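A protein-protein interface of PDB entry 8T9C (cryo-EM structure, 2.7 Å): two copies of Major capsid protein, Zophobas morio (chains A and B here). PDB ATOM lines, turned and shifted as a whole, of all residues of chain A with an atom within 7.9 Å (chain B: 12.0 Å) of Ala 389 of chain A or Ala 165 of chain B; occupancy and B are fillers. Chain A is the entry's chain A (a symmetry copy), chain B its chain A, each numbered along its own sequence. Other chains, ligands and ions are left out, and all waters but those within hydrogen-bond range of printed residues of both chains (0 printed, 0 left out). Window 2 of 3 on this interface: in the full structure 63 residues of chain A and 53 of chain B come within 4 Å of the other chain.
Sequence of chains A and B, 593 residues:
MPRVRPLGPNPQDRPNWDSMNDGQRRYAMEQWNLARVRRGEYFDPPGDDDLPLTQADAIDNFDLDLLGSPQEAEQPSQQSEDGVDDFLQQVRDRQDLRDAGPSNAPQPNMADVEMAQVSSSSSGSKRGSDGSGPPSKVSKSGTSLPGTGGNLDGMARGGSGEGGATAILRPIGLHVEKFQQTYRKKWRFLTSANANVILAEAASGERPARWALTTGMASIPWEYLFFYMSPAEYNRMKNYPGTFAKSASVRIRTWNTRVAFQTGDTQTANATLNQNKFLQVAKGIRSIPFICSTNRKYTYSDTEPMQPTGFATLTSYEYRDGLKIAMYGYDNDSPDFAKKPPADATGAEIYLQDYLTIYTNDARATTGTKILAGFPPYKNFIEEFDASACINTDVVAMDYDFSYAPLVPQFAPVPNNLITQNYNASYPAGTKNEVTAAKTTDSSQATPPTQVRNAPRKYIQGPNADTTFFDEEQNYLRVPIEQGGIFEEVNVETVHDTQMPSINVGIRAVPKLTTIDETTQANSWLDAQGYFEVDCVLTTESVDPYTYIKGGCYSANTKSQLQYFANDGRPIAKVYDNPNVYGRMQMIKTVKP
O of Thr 166 of chain B is in hydrogen-bond range of N of Asp 386 of chain A (3.5 Å). The backbone NH (N) of Ile 168 of chain B lies within hydrogen-bond range of the backbone carbonyl oxygen (O) of Glu 384 of chain A, at 3.0 Å. The backbone NH of Glu 384 of chain A sits at hydrogen-bond distance from the backbone carbonyl oxygen of Leu 169 of chain B (3.1 Å).
The backbone NH (N) of Leu 279 of chain A sits at hydrogen-bond distance from the backbone carbonyl oxygen (O) of Phe 385 of chain A. The backbone NH (N) of Ala 389 of chain A sits at hydrogen-bond distance from the side-chain carboxylate (OD1) of Asp 386 of chain A (3.5 Å). SG of Cys 390 of chain A sits at hydrogen-bond distance from O of Asp 386 of chain A, 3.3 Å away. The backbone carbonyl oxygen (O) of Cys 390 of chain A is in hydrogen-bond range of the side-chain hydroxyl (OG1) of Thr 393 of chain A (2.5 Å).
Among the printed residues, pairs that only touch across the chains: Glu 384 of chain A with Ala 167 of chain B (3.3 Å), Phe 385 of chain A with Ala 165 of chain B (3.9 Å), Phe 385 of chain A with Thr 166 of chain B (3.7 Å), Phe 385 of chain A with Ala 167 of chain B (3.9 Å), Ala 389 of chain A with Ala 165 of chain B (3.8 Å) and Cys 390 of chain A with Ala 165 of chain B (3.4 Å).
Printed residues of chain B within 4 Å of Glu 384 of chain A: Ala 167, Ile 168 and Leu 169. Phe 385 of chain A touches just these residues of chain B: Ala 165, Thr 166 and Ala 167. Of chain B, only Thr 166 comes within 4 Å of Asp 386 of chain A. Ala 387 of chain A touches none of the printed residues of chain B. Ser 388 of chain A touches none of the printed residues of chain B. Of chain B, only Ala 165 (3.8 Å) comes within 4 Å of Ala 389 of chain A. Of the printed residues of chain B, Cys 390 of chain A touches Ala 165. No residue of chain B comes within 4 Å of Ile 391 of chain A. No residue of chain B comes within 4 Å of Thr 393 of chain A. Of chain A, only Phe 385 (3.9 Å), Ala 389 (3.8 Å) and Cys 390 (3.4 Å) come within 4 Å of Ala 165 of chain B. Printed residues of chain A within 4 Å of Thr 166 of chain B: Phe 385 (3.7 Å) and Asp 386 (3.5 Å). Printed residues of chain A within 4 Å of Ala 167 of chain B: Glu 384 and Phe 385. Of the printed residues of chain A, Leu 169 of chain B touches Glu 384 (3.1 Å). The nearest residue of chain A that does not touch Ala 165 of chain B is Asp 386 of chain A (4.1 Å).
Of the 15 printed residues of chain A, 5 touch a printed residue of chain B. Along chain B the printed residues that touch a printed residue of chain A span positions 165 to 169. Among the printed residues, 9 pairs touch across the chains. Among the printed residues, no Asp or Glu carboxylate lies within 4 Å of a Lys or Arg side-chain nitrogen of the other chain.
No position is printed for both chains. Of the 9 pairs that touch across the chains among the printed residues, none has its exchanged pair printed and touching as well.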
ATOM      1  N   THR A 254       9.720 -11.622  27.167  1.00  0.00           N
ATOM      2  CA  THR A 254       9.997 -12.869  26.472  1.00  0.00           C
ATOM      3  C   THR A 254       9.512 -12.790  25.030  1.00  0.00           C
ATOM      4  O   THR A 254       8.476 -12.186  24.738  1.00  0.00           O
ATOM      5  CB  THR A 254       9.355 -14.059  27.193  1.00  0.00           C
ATOM      6  OG1 THR A 254       9.768 -15.278  26.564  1.00  0.00           O
ATOM      7  CG2 THR A 254       7.843 -13.970  27.180  1.00  0.00           C
ATOM      8  N   ASN A 256       9.353 -15.125  21.082  1.00  0.00           N
ATOM      9  CA  ASN A 256       8.909 -16.444  20.648  1.00  0.00           C
ATOM     10  C   ASN A 256       9.829 -17.526  21.198  1.00  0.00           C
ATOM     11  O   ASN A 256      11.056 -17.413  21.132  1.00  0.00           O
ATOM     12  CB  ASN A 256       8.868 -16.508  19.122  1.00  0.00           C
ATOM     13  CG  ASN A 256       8.073 -17.692  18.609  1.00  0.00           C
ATOM     14  OD1 ASN A 256       7.266 -18.271  19.333  1.00  0.00           O
ATOM     15  ND2 ASN A 256       8.296 -18.055  17.353  1.00  0.00           N
ATOM     16  N   LYS A 277       3.704 -25.408  25.399  1.00  0.00           N
ATOM     17  CA  LYS A 277       4.860 -24.536  25.575  1.00  0.00           C
ATOM     18  C   LYS A 277       4.585 -23.604  26.743  1.00  0.00           C
ATOM     19  O   LYS A 277       3.717 -22.731  26.646  1.00  0.00           O
ATOM     20  CB  LYS A 277       5.117 -23.760  24.288  1.00  0.00           C
ATOM     21  CG  LYS A 277       6.467 -23.118  24.169  1.00  0.00           C
ATOM     22  CD  LYS A 277       6.464 -22.154  23.000  1.00  0.00           C
ATOM     23  CE  LYS A 277       6.184 -22.876  21.694  1.00  0.00           C
ATOM     24  NZ  LYS A 277       6.552 -22.046  20.517  1.00  0.00           N
ATOM     25  N   LEU A 279       6.048 -21.095  30.040  1.00  0.00           N
ATOM     26  CA  LEU A 279       7.094 -20.241  30.586  1.00  0.00           C
ATOM     27  C   LEU A 279       6.939 -20.160  32.097  1.00  0.00           C
ATOM     28  O   LEU A 279       5.838 -19.920  32.599  1.00  0.00           O
ATOM     29  CB  LEU A 279       7.026 -18.847  29.962  1.00  0.00           C
ATOM     30  CG  LEU A 279       7.589 -17.656  30.738  1.00  0.00           C
ATOM     31  CD1 LEU A 279       9.094 -17.747  30.882  1.00  0.00           C
ATOM     32  CD2 LEU A 279       7.201 -16.367  30.048  1.00  0.00           C
ATOM     33  N   GLU A 384       3.409 -19.842  35.980  1.00  0.00           N
ATOM     34  CA  GLU A 384       3.608 -20.540  34.721  1.00  0.00           C
ATOM     35  C   GLU A 384       2.512 -20.124  33.754  1.00  0.00           C
ATOM     36  O   GLU A 384       1.338 -20.062  34.125  1.00  0.00           O
ATOM     37  CB  GLU A 384       3.609 -22.057  34.923  1.00  0.00           C
ATOM     38  CG  GLU A 384       4.047 -22.853  33.714  1.00  0.00           C
ATOM     39  CD  GLU A 384       4.869 -24.061  34.092  1.00  0.00           C
ATOM     40  OE1 GLU A 384       5.228 -24.186  35.280  1.00  0.00           O
ATOM     41  OE2 GLU A 384       5.152 -24.891  33.206  1.00  0.00           O
ATOM     42  N   PHE A 385       2.903 -19.832  32.517  1.00  0.00           N
ATOM     43  CA  PHE A 385       1.983 -19.352  31.496  1.00  0.00           C
ATOM     44  C   PHE A 385       2.242 -20.093  30.197  1.00  0.00           C
ATOM     45  O   PHE A 385       3.334 -20.613  29.970  1.00  0.00           O
ATOM     46  CB  PHE A 385       2.129 -17.844  31.248  1.00  0.00           C
ATOM     47  CG  PHE A 385       2.318 -17.032  32.493  1.00  0.00           C
ATOM     48  CD1 PHE A 385       1.225 -16.561  33.200  1.00  0.00           C
ATOM     49  CD2 PHE A 385       3.587 -16.732  32.956  1.00  0.00           C
ATOM     50  CE1 PHE A 385       1.394 -15.812  34.345  1.00  0.00           C
ATOM     51  CE2 PHE A 385       3.761 -15.982  34.101  1.00  0.00           C
ATOM     52  CZ  PHE A 385       2.662 -15.521  34.795  1.00  0.00           C
ATOM     53  N   ASP A 386       1.223 -20.129  29.342  1.00  0.00           N
ATOM     54  CA  ASP A 386       1.386 -20.685  28.005  1.00  0.00           C
ATOM     55  C   ASP A 386       2.307 -19.780  27.196  1.00  0.00           C
ATOM     56  O   ASP A 386       1.941 -18.649  26.861  1.00  0.00           O
ATOM     57  CB  ASP A 386       0.029 -20.830  27.325  1.00  0.00           C
ATOM     58  CG  ASP A 386       0.127 -21.477  25.958  1.00  0.00           C
ATOM     59  OD1 ASP A 386      -0.142 -20.789  24.953  1.00  0.00           O
ATOM     60  OD2 ASP A 386       0.481 -22.672  25.889  1.00  0.00           O
ATOM     61  N   ALA A 387       3.507 -20.278  26.885  1.00  0.00           N
ATOM     62  CA  ALA A 387       4.515 -19.436  26.247  1.00  0.00           C
ATOM     63  C   ALA A 387       4.111 -19.036  24.835  1.00  0.00           C
ATOM     64  O   ALA A 387       4.665 -18.079  24.282  1.00  0.00           O
ATOM     65  CB  ALA A 387       5.864 -20.151  26.232  1.00  0.00           C
ATOM     66  N   SER A 388       3.160 -19.752  24.233  1.00  0.00           N
ATOM     67  CA  SER A 388       2.669 -19.360  22.917  1.00  0.00           C
ATOM     68  C   SER A 388       1.905 -18.046  22.978  1.00  0.00           C
ATOM     69  O   SER A 388       1.877 -17.296  21.996  1.00  0.00           O
ATOM     70  CB  SER A 388       1.787 -20.462  22.335  1.00  0.00           C
ATOM     71  OG  SER A 388       2.379 -21.737  22.513  1.00  0.00           O
ATOM     72  N   ALA A 389       1.278 -17.750  24.116  1.00  0.00           N
ATOM     73  CA  ALA A 389       0.531 -16.513  24.291  1.00  0.00           C
ATOM     74  C   ALA A 389       1.378 -15.371  24.835  1.00  0.00           C
ATOM     75  O   ALA A 389       0.882 -14.245  24.924  1.00  0.00           O
ATOM     76  CB  ALA A 389      -0.659 -16.750  25.221  1.00  0.00           C
ATOM     77  N   CYS A 390       2.632 -15.629  25.197  1.00  0.00           N
ATOM     78  CA  CYS A 390       3.482 -14.630  25.826  1.00  0.00           C
ATOM     79  C   CYS A 390       4.490 -14.003  24.874  1.00  0.00           C
ATOM     80  O   CYS A 390       5.400 -13.309  25.331  1.00  0.00           O
ATOM     81  CB  CYS A 390       4.219 -15.242  27.020  1.00  0.00           C
ATOM     82  SG  CYS A 390       3.135 -15.900  28.301  1.00  0.00           S
ATOM     83  N   ILE A 391       4.351 -14.222  23.564  1.00  0.00           N
ATOM     84  CA  ILE A 391       5.330 -13.701  22.617  1.00  0.00           C
ATOM     85  C   ILE A 391       5.310 -12.179  22.642  1.00  0.00           C
ATOM     86  O   ILE A 391       4.258 -11.551  22.476  1.00  0.00           O
ATOM     87  CB  ILE A 391       5.053 -14.244  21.208  1.00  0.00           C
ATOM     88  CG1 ILE A 391       4.924 -15.766  21.245  1.00  0.00           C
ATOM     89  CG2 ILE A 391       6.156 -13.822  20.252  1.00  0.00           C
ATOM     90  CD1 ILE A 391       4.549 -16.377  19.916  1.00  0.00           C
ATOM     91  N   ASN A 392       6.486 -11.586  22.847  1.00  0.00           N
ATOM     92  CA  ASN A 392       6.653 -10.137  22.961  1.00  0.00           C
ATOM     93  C   ASN A 392       5.715  -9.571  24.029  1.00  0.00           C
ATOM     94  O   ASN A 392       4.832  -8.755  23.764  1.00  0.00           O
ATOM     95  CB  ASN A 392       6.451  -9.456  21.602  1.00  0.00           C
ATOM     96  CG  ASN A 392       6.504  -7.938  21.686  1.00  0.00           C
ATOM     97  OD1 ASN A 392       7.564  -7.334  21.522  1.00  0.00           O
ATOM     98  ND2 ASN A 392       5.359  -7.318  21.939  1.00  0.00           N
ATOM     99  N   THR A 393       5.899 -10.045  25.259  1.00  0.00           N
ATOM    100  CA  THR A 393       5.118  -9.588  26.398  1.00  0.00           C
ATOM    101  C   THR A 393       6.033  -9.446  27.603  1.00  0.00           C
ATOM    102  O   THR A 393       6.952 -10.246  27.790  1.00  0.00           O
ATOM    103  CB  THR A 393       3.971 -10.555  26.745  1.00  0.00           C
ATOM    104  OG1 THR A 393       4.511 -11.837  27.088  1.00  0.00           O
ATOM    105  CG2 THR A 393       2.999 -10.709  25.581  1.00  0.00           C
ATOM    106  N   VAL A 395       7.112  -9.987  31.244  1.00  0.00           N
ATOM    107  CA  VAL A 395       6.853 -11.039  32.217  1.00  0.00           C
ATOM    108  C   VAL A 395       7.402 -10.720  33.601  1.00  0.00           C
ATOM    109  O   VAL A 395       6.838 -11.201  34.596  1.00  0.00           O
ATOM    110  CB  VAL A 395       7.403 -12.396  31.729  1.00  0.00           C
ATOM    111  CG1 VAL A 395       6.717 -12.806  30.445  1.00  0.00           C
ATOM    112  CG2 VAL A 395       8.910 -12.329  31.528  1.00  0.00           C
ATOM    113  N   ALA B 165      -2.090 -14.226  28.686  1.00  0.00           N
ATOM    114  CA  ALA B 165      -1.719 -15.636  28.716  1.00  0.00           C
ATOM    115  C   ALA B 165      -2.435 -16.360  29.849  1.00  0.00           C
ATOM    116  O   ALA B 165      -2.601 -15.810  30.937  1.00  0.00           O
ATOM    117  CB  ALA B 165      -0.215 -15.786  28.859  1.00  0.00           C
ATOM    118  N   THR B 166      -2.853 -17.596  29.592  1.00  0.00           N
ATOM    119  CA  THR B 166      -3.571 -18.382  30.589  1.00  0.00           C
ATOM    120  C   THR B 166      -2.566 -18.969  31.570  1.00  0.00           C
ATOM    121  O   THR B 166      -1.710 -19.774  31.190  1.00  0.00           O
ATOM    122  CB  THR B 166      -4.397 -19.480  29.922  1.00  0.00           C
ATOM    123  OG1 THR B 166      -3.556 -20.267  29.070  1.00  0.00           O
ATOM    124  CG2 THR B 166      -5.515 -18.868  29.095  1.00  0.00           C
ATOM    125  N   ALA B 167      -2.669 -18.564  32.833  1.00  0.00           N
ATOM    126  CA  ALA B 167      -1.738 -19.009  33.864  1.00  0.00           C
ATOM    127  C   ALA B 167      -2.063 -20.442  34.262  1.00  0.00           C
ATOM    128  O   ALA B 167      -3.014 -20.685  35.013  1.00  0.00           O
ATOM    129  CB  ALA B 167      -1.807 -18.079  35.069  1.00  0.00           C
ATOM    130  N   ILE B 168      -1.278 -21.395  33.760  1.00  0.00           N
ATOM    131  CA  ILE B 168      -1.478 -22.786  34.149  1.00  0.00           C
ATOM    132  C   ILE B 168      -1.078 -23.005  35.604  1.00  0.00           C
ATOM    133  O   ILE B 168      -1.635 -23.875  36.283  1.00  0.00           O
ATOM    134  CB  ILE B 168      -0.723 -23.725  33.188  1.00  0.00           C
ATOM    135  CG1 ILE B 168      -0.969 -25.190  33.557  1.00  0.00           C
ATOM    136  CG2 ILE B 168       0.755 -23.390  33.155  1.00  0.00           C
ATOM    137  CD1 ILE B 168      -0.868 -26.140  32.388  1.00  0.00           C
ATOM    138  N   LEU B 169      -0.126 -22.228  36.115  1.00  0.00           N
ATOM    139  CA  LEU B 169       0.245 -22.279  37.521  1.00  0.00           C
ATOM    140  C   LEU B 169       0.314 -20.869  38.090  1.00  0.00           C
ATOM    141  O   LEU B 169       0.671 -19.916  37.394  1.00  0.00           O
ATOM    142  CB  LEU B 169       1.592 -22.983  37.737  1.00  0.00           C
ATOM    143  CG  LEU B 169       1.665 -24.483  37.450  1.00  0.00           C
ATOM    144  CD1 LEU B 169       3.062 -25.009  37.727  1.00  0.00           C
ATOM    145  CD2 LEU B 169       0.636 -25.235  38.271  1.00  0.00           C
ATOM    146  N   ARG B 170       0.005 -20.763  39.382  1.00  0.00           N
ATOM    147  CA  ARG B 170       0.096 -19.489  40.080  1.00  0.00           C
ATOM    148  C   ARG B 170       0.570 -19.815  41.491  1.00  0.00           C
ATOM    149  O   ARG B 170       0.334 -20.920  41.978  1.00  0.00           O
ATOM    150  CB  ARG B 170      -1.244 -18.768  40.112  1.00  0.00           C
ATOM    151  CG  ARG B 170      -1.726 -18.276  38.759  1.00  0.00           C
ATOM    152  CD  ARG B 170      -2.778 -17.189  38.914  1.00  0.00           C
ATOM    153  NE  ARG B 170      -2.234 -15.993  39.553  1.00  0.00           N
ATOM    154  CZ  ARG B 170      -2.302 -15.741  40.857  1.00  0.00           C
ATOM    155  NH1 ARG B 170      -1.776 -14.627  41.346  1.00  0.00           N
ATOM    156  NH2 ARG B 170      -2.900 -16.599  41.673  1.00  0.00           N
ATOM    157  N   PRO B 171       1.239 -18.869  42.160  1.00  0.00           N
ATOM    158  CA  PRO B 171       1.803 -19.129  43.500  1.00  0.00           C
ATOM    159  C   PRO B 171       0.725 -19.195  44.574  1.00  0.00           C
ATOM    160  O   PRO B 171       0.447 -18.237  45.303  1.00  0.00           O
ATOM    161  CB  PRO B 171       2.759 -17.944  43.692  1.00  0.00           C
ATOM    162  CG  PRO B 171       2.928 -17.330  42.342  1.00  0.00           C
ATOM    163  CD  PRO B 171       1.634 -17.549  41.655  1.00  0.00           C
